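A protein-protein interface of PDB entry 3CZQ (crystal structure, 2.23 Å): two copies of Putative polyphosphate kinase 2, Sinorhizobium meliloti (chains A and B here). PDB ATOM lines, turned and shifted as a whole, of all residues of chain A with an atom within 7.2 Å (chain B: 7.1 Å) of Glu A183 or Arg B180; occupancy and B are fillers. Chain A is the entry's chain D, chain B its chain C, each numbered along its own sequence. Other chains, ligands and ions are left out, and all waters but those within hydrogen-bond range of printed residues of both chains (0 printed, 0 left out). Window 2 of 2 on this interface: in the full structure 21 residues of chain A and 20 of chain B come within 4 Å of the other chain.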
ATOM      1  N   GLU A 177     -14.432  15.192   1.526  1.00  0.00           N
ATOM      2  CA  GLU A 177     -15.794  14.905   2.020  1.00  0.00           C
ATOM      3  C   GLU A 177     -16.205  13.436   2.127  1.00  0.00           C
ATOM      4  O   GLU A 177     -17.053  13.105   2.954  1.00  0.00           O
ATOM      5  CB  GLU A 177     -16.863  15.702   1.252  1.00  0.00           C
ATOM      6  CG  GLU A 177     -16.817  17.215   1.500  1.00  0.00           C
ATOM      7  CD  GLU A 177     -17.023  17.595   2.971  1.00  0.00           C
ATOM      8  OE1 GLU A 177     -18.050  17.209   3.574  1.00  0.00           O
ATOM      9  OE2 GLU A 177     -16.155  18.299   3.530  1.00  0.00           O
ATOM     10  N   ALA A 178     -15.602  12.556   1.316  1.00  0.00           N
ATOM     11  CA  ALA A 178     -15.998  11.133   1.294  1.00  0.00           C
ATOM     12  C   ALA A 178     -15.705  10.340   2.573  1.00  0.00           C
ATOM     13  O   ALA A 178     -16.438   9.413   2.881  1.00  0.00           O
ATOM     14  CB  ALA A 178     -15.431  10.395   0.055  1.00  0.00           C
ATOM     15  N   PRO A 179     -14.605  10.650   3.290  1.00  0.00           N
ATOM     16  CA  PRO A 179     -14.469   9.984   4.601  1.00  0.00           C
ATOM     17  C   PRO A 179     -15.516  10.429   5.658  1.00  0.00           C
ATOM     18  O   PRO A 179     -15.977   9.601   6.454  1.00  0.00           O
ATOM     19  CB  PRO A 179     -13.013  10.318   5.025  1.00  0.00           C
ATOM     20  CG  PRO A 179     -12.327  10.823   3.756  1.00  0.00           C
ATOM     21  CD  PRO A 179     -13.424  11.486   2.980  1.00  0.00           C
ATOM     22  N   ARG A 180     -15.893  11.709   5.651  1.00  0.00           N
ATOM     23  CA  ARG A 180     -17.002  12.212   6.492  1.00  0.00           C
ATOM     24  C   ARG A 180     -18.333  11.522   6.161  1.00  0.00           C
ATOM     25  O   ARG A 180     -19.094  11.150   7.062  1.00  0.00           O
ATOM     26  CB  ARG A 180     -17.149  13.741   6.375  1.00  0.00           C
ATOM     27  CG  ARG A 180     -15.932  14.507   6.812  1.00  0.00           C
ATOM     28  CD  ARG A 180     -16.208  15.985   7.061  1.00  0.00           C
ATOM     29  NE  ARG A 180     -14.956  16.681   7.362  1.00  0.00           N
ATOM     30  CZ  ARG A 180     -14.274  17.422   6.489  1.00  0.00           C
ATOM     31  NH1 ARG A 180     -14.735  17.594   5.260  1.00  0.00           N
ATOM     32  NH2 ARG A 180     -13.132  18.005   6.843  1.00  0.00           N
ATOM     33  N   PHE A 181     -18.593  11.353   4.862  1.00  0.00           N
ATOM     34  CA  PHE A 181     -19.761  10.611   4.357  1.00  0.00           C
ATOM     35  C   PHE A 181     -19.760   9.182   4.893  1.00  0.00           C
ATOM     36  O   PHE A 181     -20.741   8.710   5.454  1.00  0.00           O
ATOM     37  CB  PHE A 181     -19.718  10.600   2.828  1.00  0.00           C
ATOM     38  CG  PHE A 181     -20.959  10.031   2.162  1.00  0.00           C
ATOM     39  CD1 PHE A 181     -22.211  10.615   2.356  1.00  0.00           C
ATOM     40  CD2 PHE A 181     -20.855   8.950   1.283  1.00  0.00           C
ATOM     41  CE1 PHE A 181     -23.342  10.103   1.715  1.00  0.00           C
ATOM     42  CE2 PHE A 181     -21.988   8.434   0.641  1.00  0.00           C
ATOM     43  CZ  PHE A 181     -23.222   9.012   0.853  1.00  0.00           C
ATOM     44  N   GLU A 182     -18.623   8.519   4.737  1.00  0.00           N
ATOM     45  CA  GLU A 182     -18.462   7.136   5.159  1.00  0.00           C
ATOM     46  C   GLU A 182     -18.487   6.983   6.675  1.00  0.00           C
ATOM     47  O   GLU A 182     -18.918   5.948   7.182  1.00  0.00           O
ATOM     48  CB  GLU A 182     -17.198   6.550   4.533  1.00  0.00           C
ATOM     49  CG  GLU A 182     -17.326   6.495   3.002  1.00  0.00           C
ATOM     50  CD  GLU A 182     -16.108   5.954   2.261  1.00  0.00           C
ATOM     51  OE1 GLU A 182     -15.130   5.519   2.912  1.00  0.00           O
ATOM     52  OE2 GLU A 182     -16.145   5.960   1.006  1.00  0.00           O
ATOM     53  N   GLU A 183     -18.046   8.018   7.390  1.00  0.00           N
ATOM     54  CA  GLU A 183     -18.199   8.067   8.845  1.00  0.00           C
ATOM     55  C   GLU A 183     -19.671   7.995   9.269  1.00  0.00           C
ATOM     56  O   GLU A 183     -20.014   7.171  10.120  1.00  0.00           O
ATOM     57  CB  GLU A 183     -17.527   9.300   9.451  1.00  0.00           C
ATOM     58  CG  GLU A 183     -17.785   9.410  10.957  1.00  0.00           C
ATOM     59  CD  GLU A 183     -16.860  10.381  11.700  1.00  0.00           C
ATOM     60  OE1 GLU A 183     -15.665  10.463  11.352  1.00  0.00           O
ATOM     61  OE2 GLU A 183     -17.334  11.047  12.649  1.00  0.00           O
ATOM     62  N   MET A 184     -20.527   8.832   8.666  1.00  0.00           N
ATOM     63  CA  MET A 184     -21.969   8.794   8.940  1.00  0.00           C
ATOM     64  C   MET A 184     -22.634   7.469   8.548  1.00  0.00           C
ATOM     65  O   MET A 184     -23.571   7.026   9.222  1.00  0.00           O
ATOM     66  CB  MET A 184     -22.730   9.968   8.278  1.00  0.00           C
ATOM     67  CG  MET A 184     -22.239  11.367   8.644  1.00  0.00           C
ATOM     68  SD  MET A 184     -23.499  12.806   8.178  1.00  0.00           S
ATOM     69  CE  MET A 184     -24.820  12.462   9.576  1.00  0.00           C
ATOM     70  N   ILE A 185     -22.174   6.866   7.448  1.00  0.00           N
ATOM     71  CA  ILE A 185     -22.669   5.556   7.006  1.00  0.00           C
ATOM     72  C   ILE A 185     -22.361   4.534   8.097  1.00  0.00           C
ATOM     73  O   ILE A 185     -23.267   3.850   8.580  1.00  0.00           O
ATOM     74  CB  ILE A 185     -22.061   5.117   5.642  1.00  0.00           C
ATOM     75  CG1 ILE A 185     -22.594   5.977   4.494  1.00  0.00           C
ATOM     76  CG2 ILE A 185     -22.331   3.625   5.358  1.00  0.00           C
ATOM     77  CD1 ILE A 185     -21.697   5.938   3.228  1.00  0.00           C
ATOM     78  N   ALA A 186     -21.083   4.451   8.490  1.00  0.00           N
ATOM     79  CA  ALA A 186     -20.634   3.585   9.583  1.00  0.00           C
ATOM     80  C   ALA A 186     -21.358   3.902  10.918  1.00  0.00           C
ATOM     81  O   ALA A 186     -21.829   2.986  11.600  1.00  0.00           O
ATOM     82  CB  ALA A 186     -19.140   3.687   9.744  1.00  0.00           C
ATOM     83  N   ASN A 187     -21.468   5.180  11.276  1.00  0.00           N
ATOM     84  CA  ASN A 187     -22.176   5.572  12.510  1.00  0.00           C
ATOM     85  C   ASN A 187     -23.599   5.032  12.614  1.00  0.00           C
ATOM     86  O   ASN A 187     -24.069   4.690  13.711  1.00  0.00           O
ATOM     87  CB  ASN A 187     -22.156   7.096  12.699  1.00  0.00           C
ATOM     88  CG  ASN A 187     -20.812   7.587  13.203  1.00  0.00           C
ATOM     89  OD1 ASN A 187     -19.993   6.793  13.641  1.00  0.00           O
ATOM     90  ND2 ASN A 187     -20.573   8.886  13.118  1.00  0.00           N
ATOM     91  N   GLU A 188     -24.255   4.953  11.450  1.00  0.00           N
ATOM     92  CA  GLU A 188     -25.601   4.417  11.285  1.00  0.00           C
ATOM     93  C   GLU A 188     -25.641   2.890  11.400  1.00  0.00           C
ATOM     94  O   GLU A 188     -26.691   2.308  11.670  1.00  0.00           O
ATOM     95  CB  GLU A 188     -26.159   4.876   9.928  1.00  0.00           C
ATOM     96  CG  GLU A 188     -27.448   4.192   9.462  1.00  0.00           C
ATOM     97  CD  GLU A 188     -28.674   4.668  10.205  1.00  0.00           C
ATOM     98  OE1 GLU A 188     -28.603   5.741  10.811  1.00  0.00           O
ATOM     99  OE2 GLU A 188     -29.717   3.987  10.188  1.00  0.00           O
ATOM    100  N   GLY A 189     -24.504   2.236  11.176  1.00  0.00           N
ATOM    101  CA  GLY A 189     -24.432   0.782  11.270  1.00  0.00           C
ATOM    102  C   GLY A 189     -24.655   0.051   9.955  1.00  0.00           C
ATOM    103  O   GLY A 189     -24.796  -1.177   9.932  1.00  0.00           O
ATOM    104  N   LEU A 192     -20.086  -0.837   5.262  1.00  0.00           N
ATOM    105  CA  LEU A 192     -19.585  -0.447   3.955  1.00  0.00           C
ATOM    106  C   LEU A 192     -18.290  -1.145   3.544  1.00  0.00           C
ATOM    107  O   LEU A 192     -17.213  -0.934   4.155  1.00  0.00           O
ATOM    108  CB  LEU A 192     -19.422   1.065   3.840  1.00  0.00           C
ATOM    109  CG  LEU A 192     -18.792   1.580   2.540  1.00  0.00           C
ATOM    110  CD1 LEU A 192     -19.739   1.398   1.351  1.00  0.00           C
ATOM    111  CD2 LEU A 192     -18.384   3.030   2.670  1.00  0.00           C
ATOM    112  N   THR A 248      -9.878   4.996   5.293  1.00  0.00           N
ATOM    113  CA  THR A 248      -9.993   5.380   6.701  1.00  0.00           C
ATOM    114  C   THR A 248     -10.423   4.171   7.526  1.00  0.00           C
ATOM    115  O   THR A 248     -10.598   3.083   6.991  1.00  0.00           O
ATOM    116  CB  THR A 248     -10.986   6.540   6.889  1.00  0.00           C
ATOM    117  OG1 THR A 248     -12.310   6.083   6.591  1.00  0.00           O
ATOM    118  CG2 THR A 248     -10.637   7.691   5.959  1.00  0.00           C
ATOM    119  N   HIS A 250     -13.288   3.790   9.421  1.00  0.00           N
ATOM    120  CA  HIS A 250     -14.720   3.504   9.277  1.00  0.00           C
ATOM    121  C   HIS A 250     -15.064   3.085   7.847  1.00  0.00           C
ATOM    122  O   HIS A 250     -16.038   2.357   7.635  1.00  0.00           O
ATOM    123  CB  HIS A 250     -15.582   4.699   9.729  1.00  0.00           C
ATOM    124  CG  HIS A 250     -15.095   6.016   9.214  1.00  0.00           C
ATOM    125  ND1 HIS A 250     -14.337   6.882   9.978  1.00  0.00           N
ATOM    126  CD2 HIS A 250     -15.216   6.595   7.996  1.00  0.00           C
ATOM    127  CE1 HIS A 250     -14.028   7.946   9.255  1.00  0.00           C
ATOM    128  NE2 HIS A 250     -14.547   7.792   8.046  1.00  0.00           N
ATOM    129  N   GLY A 251     -14.263   3.551   6.883  1.00  0.00           N
ATOM    130  CA  GLY A 251     -14.331   3.088   5.482  1.00  0.00           C
ATOM    131  C   GLY A 251     -13.000   2.608   4.893  1.00  0.00           C
ATOM    132  O   GLY A 251     -12.367   3.327   4.107  1.00  0.00           O
ATOM    133  N   GLN B 173     -28.033   9.349  19.435  1.00  0.00           N
ATOM    134  CA  GLN B 173     -27.350   9.331  18.135  1.00  0.00           C
ATOM    135  C   GLN B 173     -27.631  10.565  17.287  1.00  0.00           C
ATOM    136  O   GLN B 173     -26.711  11.104  16.665  1.00  0.00           O
ATOM    137  CB  GLN B 173     -27.659   8.059  17.340  1.00  0.00           C
ATOM    138  CG  GLN B 173     -26.527   7.028  17.381  1.00  0.00           C
ATOM    139  CD  GLN B 173     -25.308   7.426  16.540  1.00  0.00           C
ATOM    140  OE1 GLN B 173     -24.237   7.754  17.080  1.00  0.00           O
ATOM    141  NE2 GLN B 173     -25.472   7.401  15.210  1.00  0.00           N
ATOM    142  N   PHE B 174     -28.891  11.014  17.264  1.00  0.00           N
ATOM    143  CA  PHE B 174     -29.261  12.210  16.491  1.00  0.00           C
ATOM    144  C   PHE B 174     -28.545  13.474  16.953  1.00  0.00           C
ATOM    145  O   PHE B 174     -28.096  14.271  16.123  1.00  0.00           O
ATOM    146  CB  PHE B 174     -30.754  12.492  16.500  1.00  0.00           C
ATOM    147  CG  PHE B 174     -31.096  13.819  15.866  1.00  0.00           C
ATOM    148  CD1 PHE B 174     -31.096  13.956  14.465  1.00  0.00           C
ATOM    149  CD2 PHE B 174     -31.353  14.947  16.661  1.00  0.00           C
ATOM    150  CE1 PHE B 174     -31.366  15.176  13.871  1.00  0.00           C
ATOM    151  CE2 PHE B 174     -31.623  16.174  16.077  1.00  0.00           C
ATOM    152  CZ  PHE B 174     -31.633  16.288  14.676  1.00  0.00           C
ATOM    153  N   LEU B 175     -28.471  13.669  18.271  1.00  0.00           N
ATOM    154  CA  LEU B 175     -27.695  14.767  18.834  1.00  0.00           C
ATOM    155  C   LEU B 175     -26.231  14.675  18.385  1.00  0.00           C
ATOM    156  O   LEU B 175     -25.628  15.685  18.002  1.00  0.00           O
ATOM    157  CB  LEU B 175     -27.834  14.809  20.367  1.00  0.00           C
ATOM    158  CG  LEU B 175     -28.893  15.768  20.948  1.00  0.00           C
ATOM    159  CD1 LEU B 175     -30.294  15.633  20.321  1.00  0.00           C
ATOM    160  CD2 LEU B 175     -28.979  15.694  22.464  1.00  0.00           C
ATOM    161  N   LYS B 176     -25.679  13.462  18.394  1.00  0.00           N
ATOM    162  CA  LYS B 176     -24.319  13.244  17.911  1.00  0.00           C
ATOM    163  C   LYS B 176     -24.192  13.441  16.392  1.00  0.00           C
ATOM    164  O   LYS B 176     -23.225  14.062  15.937  1.00  0.00           O
ATOM    165  CB  LYS B 176     -23.781  11.868  18.340  1.00  0.00           C
ATOM    166  CG  LYS B 176     -22.262  11.845  18.516  1.00  0.00           C
ATOM    167  CD  LYS B 176     -21.704  10.537  19.143  1.00  0.00           C
ATOM    168  CE  LYS B 176     -21.320   9.510  18.084  1.00  0.00           C
ATOM    169  NZ  LYS B 176     -20.342   8.495  18.600  1.00  0.00           N
ATOM    170  N   GLU B 177     -25.164  12.939  15.619  1.00  0.00           N
ATOM    171  CA  GLU B 177     -25.060  12.948  14.150  1.00  0.00           C
ATOM    172  C   GLU B 177     -25.506  14.221  13.435  1.00  0.00           C
ATOM    173  O   GLU B 177     -25.064  14.471  12.304  1.00  0.00           O
ATOM    174  CB  GLU B 177     -25.723  11.710  13.517  1.00  0.00           C
ATOM    175  CG  GLU B 177     -24.992  10.401  13.805  1.00  0.00           C
ATOM    176  CD  GLU B 177     -23.523  10.439  13.386  1.00  0.00           C
ATOM    177  OE1 GLU B 177     -23.238  10.269  12.182  1.00  0.00           O
ATOM    178  OE2 GLU B 177     -22.651  10.641  14.261  1.00  0.00           O
ATOM    179  N   ALA B 178     -26.359  15.021  14.082  1.00  0.00           N
ATOM    180  CA  ALA B 178     -26.894  16.236  13.459  1.00  0.00           C
ATOM    181  C   ALA B 178     -25.846  17.278  13.025  1.00  0.00           C
ATOM    182  O   ALA B 178     -25.982  17.840  11.917  1.00  0.00           O
ATOM    183  CB  ALA B 178     -27.983  16.874  14.319  1.00  0.00           C
ATOM    184  N   PRO B 179     -24.818  17.548  13.883  1.00  0.00           N
ATOM    185  CA  PRO B 179     -23.674  18.411  13.523  1.00  0.00           C
ATOM    186  C   PRO B 179     -22.748  17.844  12.435  1.00  0.00           C
ATOM    187  O   PRO B 179     -22.217  18.613  11.630  1.00  0.00           O
ATOM    188  CB  PRO B 179     -22.893  18.552  14.844  1.00  0.00           C
ATOM    189  CG  PRO B 179     -23.815  18.097  15.916  1.00  0.00           C
ATOM    190  CD  PRO B 179     -24.707  17.086  15.282  1.00  0.00           C
ATOM    191  N   ARG B 180     -22.542  16.529  12.404  1.00  0.00           N
ATOM    192  CA  ARG B 180     -21.755  15.927  11.315  1.00  0.00           C
ATOM    193  C   ARG B 180     -22.520  16.118  10.012  1.00  0.00           C
ATOM    194  O   ARG B 180     -21.927  16.425   8.971  1.00  0.00           O
ATOM    195  CB  ARG B 180     -21.473  14.436  11.550  1.00  0.00           C
ATOM    196  CG  ARG B 180     -20.519  14.148  12.685  1.00  0.00           C
ATOM    197  CD  ARG B 180     -20.328  12.645  12.880  1.00  0.00           C
ATOM    198  NE  ARG B 180     -19.389  12.382  13.981  1.00  0.00           N
ATOM    199  CZ  ARG B 180     -19.730  11.971  15.203  1.00  0.00           C
ATOM    200  NH1 ARG B 180     -20.994  11.729  15.522  1.00  0.00           N
ATOM    201  NH2 ARG B 180     -18.793  11.782  16.115  1.00  0.00           N
ATOM    202  N   PHE B 181     -23.841  15.945  10.105  1.00  0.00           N
ATOM    203  CA  PHE B 181     -24.777  16.169   9.007  1.00  0.00           C
ATOM    204  C   PHE B 181     -24.724  17.606   8.503  1.00  0.00           C
ATOM    205  O   PHE B 181     -24.609  17.841   7.294  1.00  0.00           O
ATOM    206  CB  PHE B 181     -26.188  15.827   9.475  1.00  0.00           C
ATOM    207  CG  PHE B 181     -27.229  15.862   8.385  1.00  0.00           C
ATOM    208  CD1 PHE B 181     -27.265  14.883   7.403  1.00  0.00           C
ATOM    209  CD2 PHE B 181     -28.204  16.860   8.370  1.00  0.00           C
ATOM    210  CE1 PHE B 181     -28.238  14.915   6.418  1.00  0.00           C
ATOM    211  CE2 PHE B 181     -29.174  16.898   7.387  1.00  0.00           C
ATOM    212  CZ  PHE B 181     -29.200  15.927   6.420  1.00  0.00           C
ATOM    213  N   GLU B 182     -24.783  18.553   9.438  1.00  0.00           N
ATOM    214  CA  GLU B 182     -24.765  19.963   9.092  1.00  0.00           C
ATOM    215  C   GLU B 182     -23.384  20.491   8.673  1.00  0.00           C
ATOM    216  O   GLU B 182     -23.306  21.456   7.897  1.00  0.00           O
ATOM    217  CB  GLU B 182     -25.394  20.807  10.212  1.00  0.00           C
ATOM    218  CG  GLU B 182     -26.920  20.640  10.291  1.00  0.00           C
ATOM    219  CD  GLU B 182     -27.474  20.888  11.676  1.00  0.00           C
ATOM    220  OE1 GLU B 182     -26.896  21.728  12.383  1.00  0.00           O
ATOM    221  OE2 GLU B 182     -28.492  20.260  12.050  1.00  0.00           O
ATOM    222  N   GLU B 183     -22.303  19.861   9.152  1.00  0.00           N
ATOM    223  CA  GLU B 183     -20.980  20.173   8.607  1.00  0.00           C
ATOM    224  C   GLU B 183     -20.939  19.872   7.110  1.00  0.00           C
ATOM    225  O   GLU B 183     -20.400  20.667   6.336  1.00  0.00           O
ATOM    226  CB  GLU B 183     -19.837  19.451   9.327  1.00  0.00           C
ATOM    227  CG  GLU B 183     -18.465  19.792   8.704  1.00  0.00           C
ATOM    228  CD  GLU B 183     -17.251  19.356   9.529  1.00  0.00           C
ATOM    229  OE1 GLU B 183     -17.430  18.529  10.454  1.00  0.00           O
ATOM    230  OE2 GLU B 183     -16.113  19.825   9.231  1.00  0.00           O
ATOM    231  N   MET B 184     -21.529  18.742   6.716  1.00  0.00           N
ATOM    232  CA  MET B 184     -21.613  18.338   5.301  1.00  0.00           C
ATOM    233  C   MET B 184     -22.369  19.328   4.434  1.00  0.00           C
ATOM    234  O   MET B 184     -21.960  19.588   3.298  1.00  0.00           O
ATOM    235  CB  MET B 184     -22.190  16.921   5.155  1.00  0.00           C
ATOM    236  CG  MET B 184     -21.238  15.837   5.717  1.00  0.00           C
ATOM    237  SD  MET B 184     -21.325  14.046   4.949  1.00  0.00           S
ATOM    238  CE  MET B 184     -20.143  14.329   3.419  1.00  0.00           C
ATOM    239  N   ILE B 185     -23.460  19.869   4.987  1.00  0.00           N
ATOM    240  CA  ILE B 185     -24.286  20.890   4.353  1.00  0.00           C
ATOM    241  C   ILE B 185     -23.467  22.164   4.153  1.00  0.00           C
ATOM    242  O   ILE B 185     -23.373  22.688   3.042  1.00  0.00           O
ATOM    243  CB  ILE B 185     -25.550  21.172   5.212  1.00  0.00           C
ATOM    244  CG1 ILE B 185     -26.485  19.951   5.194  1.00  0.00           C
ATOM    245  CG2 ILE B 185     -26.259  22.493   4.795  1.00  0.00           C
ATOM    246  CD1 ILE B 185     -27.614  20.023   6.188  1.00  0.00           C
ATOM    247  N   ASN B 187     -20.228  22.427   4.231  1.00  0.00           N
ATOM    248  CA  ASN B 187     -19.065  22.159   3.387  1.00  0.00           C
ATOM    249  C   ASN B 187     -19.453  22.129   1.920  1.00  0.00           C
ATOM    250  O   ASN B 187     -18.641  22.460   1.053  1.00  0.00           O
ATOM    251  CB  ASN B 187     -18.356  20.844   3.769  1.00  0.00           C
ATOM    252  CG  ASN B 187     -17.622  20.931   5.110  1.00  0.00           C
ATOM    253  OD1 ASN B 187     -17.567  21.996   5.742  1.00  0.00           O
ATOM    254  ND2 ASN B 187     -17.064  19.803   5.554  1.00  0.00           N
ATOM    255  N   THR B 248     -23.527  24.481  16.569  1.00  0.00           N
ATOM    256  CA  THR B 248     -22.127  24.565  16.171  1.00  0.00           C
ATOM    257  C   THR B 248     -21.876  25.803  15.302  1.00  0.00           C
ATOM    258  O   THR B 248     -22.815  26.520  14.919  1.00  0.00           O
ATOM    259  CB  THR B 248     -21.671  23.298  15.386  1.00  0.00           C
ATOM    260  OG1 THR B 248     -22.233  23.323  14.068  1.00  0.00           O
ATOM    261  CG2 THR B 248     -22.085  22.014  16.105  1.00  0.00           C
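O of Asn A187 sits at hydrogen-bond distance from NE2 of Gln B173 (3.4 Å).
ND2 of Asn B187 sits close to NH1 of Arg A180.
The side-chain carboxylate (OE2) of Glu A177 is in hydrogen-bond range of the side-chain amide nitrogen (ND2) of Asn B187 (2.7 Å).
The backbone NH of Phe B181 lies close to the side-chain sulfur of Met A184, 3.7 Å away.
OE2 of Glu B183 is in salt-bridge range of NE of Arg A180.
The side-chain carboxylate (OE2) of Glu A183 lies within salt-bridge range of the guanidinium group (NE) of Arg B180 (2.8 Å).
OE2 of Glu B177 is in hydrogen-bond range of ND2 of Asn A187 (3.0 Å).
The side-chain carboxylate (OE2) of Glu B177 is in salt-bridge range of the guanidinium group (NE) of Arg B180, 3.7 Å away.
O of Lys B176 sits close to NH1 of Arg B180 (3.3 Å).
The side-chain carboxylate (OE1) of Glu A177 lies within salt-bridge range of the guanidinium group (NH1) of Arg A180 (3.7 Å).
OD1 of Asn B187 lies close to O of Glu B183 (3.2 Å).
The backbone carbonyl oxygen (O) of Glu A183 sits close to the side-chain amide nitrogen (ND2) of Asn A187 (3.5 Å).
O of Glu A177 touches CE of Met B184 (3.4 Å).
Met B184 touches Phe A181 (CE to N, 3.7 Å).
Glu B177 touches Met A184.
Met A184 touches Arg B180 (SD to C, 3.9 Å).
ND2 of Asn A187 touches NH1 of Arg B180, at 3.7 Å.
Of chain B, only Arg B180 (2.8 Å) comes within 4 Å of Glu A183.
Of the printed residues of chain A, Glu B177 touches Met A184 (3.4 Å) and Asn A187 (3.0 Å).
Of the printed residues of chain A, Glu B183 touches Arg A180 (3.8 Å).
Of the printed residues of chain B, Phe A181 touches Met B184.
His A250 touches none of the printed residues of chain B.
The nearest printed residue of chain B that does not touch Glu A177 is Glu B183 (5.0 Å).
Hydrophobic or aromatic side chains of chain A that line the printed part of chain B: Phe A181 and Met A184.
Of the 15 printed residues of chain B, 7 touch a printed residue of chain A.
Printed residues of chain B that touch a printed residue of chain A: Gln B173, Glu B177, Arg B180, Phe B181, Glu B183, Met B184 and Asn B187.
Among the printed residues, Asp or Glu carboxylates within 4 Å of a Lys or Arg side-chain nitrogen of the other chain: Arg A180 with Glu B183 (3.8 Å) and Glu A183 with Arg B180 (2.8 Å).
Glu A177 touches Met B184, and with the chains exchanged Met A184 touches Glu B177.
Glu A177 touches Asn B187, and with the chains exchanged Asn A187 touches Glu B177.
Arg A180 touches Glu B183, and with the chains exchanged Glu A183 touches Arg B180.
Arg A180 touches Asn B187, and with the chains exchanged Asn A187 touches Arg B180.
Positions printed for both chains: 177, 178, 179, 180, 181, 182, 183, 184, 185, 187 and 248.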
